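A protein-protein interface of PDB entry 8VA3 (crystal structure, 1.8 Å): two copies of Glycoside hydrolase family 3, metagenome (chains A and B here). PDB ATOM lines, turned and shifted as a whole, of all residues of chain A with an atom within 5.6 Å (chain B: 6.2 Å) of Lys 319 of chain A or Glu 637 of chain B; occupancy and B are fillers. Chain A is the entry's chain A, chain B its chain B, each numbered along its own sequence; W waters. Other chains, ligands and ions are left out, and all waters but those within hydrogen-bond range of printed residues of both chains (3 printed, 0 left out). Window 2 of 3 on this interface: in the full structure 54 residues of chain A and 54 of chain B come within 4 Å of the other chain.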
ATOM      1  N   ASP A 315     -22.130  17.766  -3.213  1.00  0.00           N
ATOM      2  CA  ASP A 315     -21.404  18.953  -3.681  1.00  0.00           C
ATOM      3  C   ASP A 315     -22.057  20.224  -3.151  1.00  0.00           C
ATOM      4  O   ASP A 315     -21.368  21.215  -2.864  1.00  0.00           O
ATOM      5  CB  ASP A 315     -21.365  19.068  -5.207  1.00  0.00           C
ATOM      6  CG  ASP A 315     -20.390  18.107  -5.877  1.00  0.00           C
ATOM      7  OD1 ASP A 315     -19.762  17.269  -5.206  1.00  0.00           O
ATOM      8  OD2 ASP A 315     -20.258  18.224  -7.113  1.00  0.00           O
ATOM      9  N   ASN A 316     -23.388  20.240  -3.089  1.00  0.00           N
ATOM     10  CA  ASN A 316     -24.073  21.454  -2.656  1.00  0.00           C
ATOM     11  C   ASN A 316     -23.692  21.838  -1.231  1.00  0.00           C
ATOM     12  O   ASN A 316     -23.635  23.027  -0.912  1.00  0.00           O
ATOM     13  CB  ASN A 316     -25.591  21.301  -2.770  1.00  0.00           C
ATOM     14  CG  ASN A 316     -26.071  21.427  -4.198  1.00  0.00           C
ATOM     15  OD1 ASN A 316     -25.406  22.068  -5.009  1.00  0.00           O
ATOM     16  ND2 ASN A 316     -27.220  20.812  -4.521  1.00  0.00           N
ATOM     17  N   LEU A 317     -23.399  20.859  -0.370  1.00  0.00           N
ATOM     18  CA  LEU A 317     -23.064  21.183   1.012  1.00  0.00           C
ATOM     19  C   LEU A 317     -21.863  22.117   1.092  1.00  0.00           C
ATOM     20  O   LEU A 317     -21.845  23.025   1.929  1.00  0.00           O
ATOM     21  CB  LEU A 317     -22.755  19.910   1.808  1.00  0.00           C
ATOM     22  CG  LEU A 317     -23.898  18.921   1.964  1.00  0.00           C
ATOM     23  CD1 LEU A 317     -23.327  17.711   2.731  1.00  0.00           C
ATOM     24  CD2 LEU A 317     -25.030  19.589   2.782  1.00  0.00           C
ATOM     25  N   TYR A 318     -20.823  21.882   0.269  1.00  0.00           N
ATOM     26  CA  TYR A 318     -19.706  22.823   0.299  1.00  0.00           C
ATOM     27  C   TYR A 318     -19.837  23.953  -0.719  1.00  0.00           C
ATOM     28  O   TYR A 318     -19.515  25.096  -0.396  1.00  0.00           O
ATOM     29  CB  TYR A 318     -18.357  22.108   0.128  1.00  0.00           C
ATOM     30  CG  TYR A 318     -17.923  21.614  -1.247  1.00  0.00           C
ATOM     31  CD1 TYR A 318     -18.448  20.427  -1.795  1.00  0.00           C
ATOM     32  CD2 TYR A 318     -16.916  22.267  -1.940  1.00  0.00           C
ATOM     33  CE1 TYR A 318     -17.995  19.944  -3.040  1.00  0.00           C
ATOM     34  CE2 TYR A 318     -16.457  21.794  -3.179  1.00  0.00           C
ATOM     35  CZ  TYR A 318     -17.005  20.643  -3.725  1.00  0.00           C
ATOM     36  OH  TYR A 318     -16.539  20.174  -4.950  1.00  0.00           O
ATOM     37  N   LYS A 319     -20.320  23.684  -1.932  1.00  0.00           N
ATOM     38  CA  LYS A 319     -20.366  24.742  -2.943  1.00  0.00           C
ATOM     39  C   LYS A 319     -21.504  25.731  -2.704  1.00  0.00           C
ATOM     40  O   LYS A 319     -21.304  26.945  -2.765  1.00  0.00           O
ATOM     41  CB  LYS A 319     -20.519  24.134  -4.332  1.00  0.00           C
ATOM     42  CG  LYS A 319     -19.276  23.428  -4.833  1.00  0.00           C
ATOM     43  CD  LYS A 319     -19.512  23.007  -6.286  1.00  0.00           C
ATOM     44  CE  LYS A 319     -18.277  22.346  -6.873  1.00  0.00           C
ATOM     45  NZ  LYS A 319     -18.516  22.037  -8.318  1.00  0.00           N
ATOM     46  N   ARG A 320     -22.719  25.230  -2.495  1.00  0.00           N
ATOM     47  CA  ARG A 320     -23.883  26.106  -2.426  1.00  0.00           C
ATOM     48  C   ARG A 320     -24.068  26.660  -1.018  1.00  0.00           C
ATOM     49  O   ARG A 320     -24.196  27.870  -0.837  1.00  0.00           O
ATOM     50  CB  ARG A 320     -25.139  25.328  -2.866  1.00  0.00           C
ATOM     51  CG  ARG A 320     -26.423  26.177  -3.028  1.00  0.00           C
ATOM     52  CD  ARG A 320     -27.674  25.231  -3.100  1.00  0.00           C
ATOM     53  NE  ARG A 320     -27.899  24.533  -1.829  1.00  0.00           N
ATOM     54  CZ  ARG A 320     -28.716  23.494  -1.652  1.00  0.00           C
ATOM     55  NH1 ARG A 320     -29.426  22.987  -2.655  1.00  0.00           N
ATOM     56  NH2 ARG A 320     -28.826  22.951  -0.438  1.00  0.00           N
ATOM     57  N   ASP A 321     -24.038  25.789  -0.010  1.00  0.00           N
ATOM     58  CA  ASP A 321     -24.445  26.201   1.332  1.00  0.00           C
ATOM     59  C   ASP A 321     -23.276  26.546   2.236  1.00  0.00           C
ATOM     60  O   ASP A 321     -23.489  27.203   3.263  1.00  0.00           O
ATOM     61  CB  ASP A 321     -25.282  25.100   1.990  1.00  0.00           C
ATOM     62  CG  ASP A 321     -26.596  24.861   1.284  1.00  0.00           C
ATOM     63  OD1 ASP A 321     -27.125  25.784   0.641  1.00  0.00           O
ATOM     64  OD2 ASP A 321     -27.129  23.734   1.378  1.00  0.00           O
ATOM     65  N   ARG A 322     -22.053  26.107   1.896  1.00  0.00           N
ATOM     66  CA  ARG A 322     -20.850  26.479   2.639  1.00  0.00           C
ATOM     67  C   ARG A 322     -20.957  26.053   4.101  1.00  0.00           C
ATOM     68  O   ARG A 322     -20.574  26.791   5.016  1.00  0.00           O
ATOM     69  CB  ARG A 322     -20.544  27.988   2.534  1.00  0.00           C
ATOM     70  CG  ARG A 322     -20.140  28.433   1.106  1.00  0.00           C
ATOM     71  CD  ARG A 322     -21.334  29.078   0.367  1.00  0.00           C
ATOM     72  NE  ARG A 322     -20.982  29.419  -1.011  1.00  0.00           N
ATOM     73  CZ  ARG A 322     -20.205  30.437  -1.353  1.00  0.00           C
ATOM     74  NH1 ARG A 322     -19.702  31.264  -0.441  1.00  0.00           N
ATOM     75  NH2 ARG A 322     -19.904  30.619  -2.639  1.00  0.00           N
ATOM     76  N   ALA A 324     -19.510  23.102   4.583  1.00  0.00           N
ATOM     77  CA  ALA A 324     -18.318  22.266   4.519  1.00  0.00           C
ATOM     78  C   ALA A 324     -17.321  23.045   3.677  1.00  0.00           C
ATOM     79  O   ALA A 324     -17.720  23.876   2.856  1.00  0.00           O
ATOM     80  CB  ALA A 324     -18.644  20.896   3.911  1.00  0.00           C
ATOM     81  N   ASN A 325     -16.036  22.803   3.888  1.00  0.00           N
ATOM     82  CA  ASN A 325     -15.026  23.550   3.139  1.00  0.00           C
ATOM     83  C   ASN A 325     -14.568  22.871   1.852  1.00  0.00           C
ATOM     84  O   ASN A 325     -13.902  23.524   1.042  1.00  0.00           O
ATOM     85  CB  ASN A 325     -13.796  23.822   4.017  1.00  0.00           C
ATOM     86  CG  ASN A 325     -14.081  24.866   5.081  1.00  0.00           C
ATOM     87  OD1 ASN A 325     -14.874  25.786   4.862  1.00  0.00           O
ATOM     88  ND2 ASN A 325     -13.438  24.734   6.227  1.00  0.00           N
ATOM     89  N   THR B 635     -23.461  33.025  -7.866  1.00  0.00           N
ATOM     90  CA  THR B 635     -22.258  33.072  -7.040  1.00  0.00           C
ATOM     91  C   THR B 635     -21.456  31.782  -7.144  1.00  0.00           C
ATOM     92  O   THR B 635     -21.996  30.684  -6.987  1.00  0.00           O
ATOM     93  CB  THR B 635     -22.635  33.340  -5.582  1.00  0.00           C
ATOM     94  OG1 THR B 635     -23.503  34.468  -5.537  1.00  0.00           O
ATOM     95  CG2 THR B 635     -21.400  33.640  -4.756  1.00  0.00           C
ATOM     96  N   MET B 636     -20.157  31.923  -7.403  1.00  0.00           N
ATOM     97  CA  MET B 636     -19.270  30.790  -7.580  1.00  0.00           C
ATOM     98  C   MET B 636     -18.600  30.399  -6.263  1.00  0.00           C
ATOM     99  O   MET B 636     -18.464  31.206  -5.341  1.00  0.00           O
ATOM    100  CB  MET B 636     -18.206  31.114  -8.634  1.00  0.00           C
ATOM    101  CG  MET B 636     -18.786  31.652  -9.943  1.00  0.00           C
ATOM    102  SD  MET B 636     -17.551  31.952 -11.234  1.00  0.00           S
ATOM    103  CE  MET B 636     -18.604  32.545 -12.570  1.00  0.00           C
ATOM    104  N   GLU B 637     -18.175  29.135  -6.197  1.00  0.00           N
ATOM    105  CA  GLU B 637     -17.431  28.608  -5.055  1.00  0.00           C
ATOM    106  C   GLU B 637     -16.293  29.540  -4.648  1.00  0.00           C
ATOM    107  O   GLU B 637     -15.505  29.981  -5.486  1.00  0.00           O
ATOM    108  CB  GLU B 637     -16.865  27.222  -5.402  1.00  0.00           C
ATOM    109  CG  GLU B 637     -15.957  26.673  -4.318  1.00  0.00           C
ATOM    110  CD  GLU B 637     -15.437  25.276  -4.603  1.00  0.00           C
ATOM    111  OE1 GLU B 637     -15.691  24.746  -5.709  1.00  0.00           O
ATOM    112  OE2 GLU B 637     -14.759  24.714  -3.718  1.00  0.00           O
ATOM    113  N   GLY B 638     -16.192  29.826  -3.353  1.00  0.00           N
ATOM    114  CA  GLY B 638     -15.111  30.674  -2.886  1.00  0.00           C
ATOM    115  C   GLY B 638     -15.320  32.167  -3.075  1.00  0.00           C
ATOM    116  O   GLY B 638     -14.427  32.949  -2.718  1.00  0.00           O
ATOM    117  N   ASN B 639     -16.441  32.589  -3.650  1.00  0.00           N
ATOM    118  CA  ASN B 639     -16.779  34.004  -3.735  1.00  0.00           C
ATOM    119  C   ASN B 639     -17.920  34.324  -2.776  1.00  0.00           C
ATOM    120  O   ASN B 639     -18.742  33.471  -2.418  1.00  0.00           O
ATOM    121  CB  ASN B 639     -17.188  34.416  -5.155  1.00  0.00           C
ATOM    122  CG  ASN B 639     -16.043  34.307  -6.165  1.00  0.00           C
ATOM    123  OD1 ASN B 639     -14.929  33.903  -5.833  1.00  0.00           O
ATOM    124  ND2 ASN B 639     -16.326  34.666  -7.412  1.00  0.00           N
HETATM  125  O   HOH W   1     -14.855  21.751  -6.183  1.00  0.00           O
HETATM  126  O   HOH W   2     -21.934  29.306  -4.663  1.00  0.00           O
HETATM  127  O   HOH W   3     -17.086  29.036  -0.833  1.00  0.00           O
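The backbone carbonyl oxygen (O) of Met 636 of chain B sits at hydrogen-bond distance from the guanidinium group (NH2) of Arg 322 of chain A. O of Asn 639 of chain B lies within hydrogen-bond range of NH2 of Arg 322 of chain A (3.1 Å).
O of Leu 317 of chain A lies within hydrogen-bond range of N of Arg 322 of chain A. The guanidinium group (NE) of Arg 322 of chain A lies within hydrogen-bond range of the backbone carbonyl oxygen (O) of Lys 319 of chain A (3.0 Å).
Tyr 318 of chain A touches Glu 637 of chain B. CE of Lys 319 of chain A touches OE1 of Glu 637 of chain B, 3.7 Å away. Arg 322 of chain A touches Thr 635 of chain B (NH2 to CG2, 3.98 Å). Arg 322 of chain A touches Glu 637 of chain B. N of Gly 638 of chain B touches NH2 of Arg 322 of chain A, at 3.9 Å.
Asn 316 of chain A touches none of the printed residues of chain B. Printed residues of chain B within 4 Å of Tyr 318 of chain A: Glu 637. Lys 319 of chain A touches just one residue of chain B: Glu 637 (3.7 Å). Arg 320 of chain A touches none of the printed residues of chain B. Of the printed residues of chain B, Arg 322 of chain A touches Thr 635 (3.98 Å), Met 636 (3.1 Å), Glu 637 (3.9996 Å), Gly 638 (3.9 Å) and Asn 639 (3.1 Å). Printed residues of chain A within 4 Å of Thr 635 of chain B: Arg 322 (3.98 Å). Of the printed residues of chain A, Glu 637 of chain B touches Tyr 318 (3.4 Å), Lys 319 (3.7 Å) and Arg 322 (3.9996 Å). Printed residues of chain A within 4 Å of Gly 638 of chain B: Arg 322 (3.9 Å).
Of the 5 printed residues of chain B, 5 touch a printed residue of chain A. Along chain B the printed residues that touch a printed residue of chain A span positions 635 to 639. Of the 10 printed residues of chain A, 3 touch a printed residue of chain B. Hydrophobic or aromatic side chains of chain A that line the printed part of chain B: Tyr 318. Among the printed residues, 7 pairs touch across the chains. Among the printed residues, no Asp or Glu carboxylate lies within 4 Å of a Lys or Arg side-chain nitrogen of the other chain.
No position is printed for both chains.
Water W1 bridges OH of Tyr 318 of chain A (2.6 Å) and OE1 of Glu 637 of chain B (3.1 Å). Water W2 lies within hydrogen-bond range of the backbone carbonyl oxygen of Thr 635 of chain B (2.7 Å), the backbone carbonyl oxygen of Lys 319 of chain A (3.1 Å) and the guanidinium group of Arg 322 of chain A (3.2 Å). Water W3 bridges N of Gly 638 of chain B and NH1 of Arg 322 of chain A.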
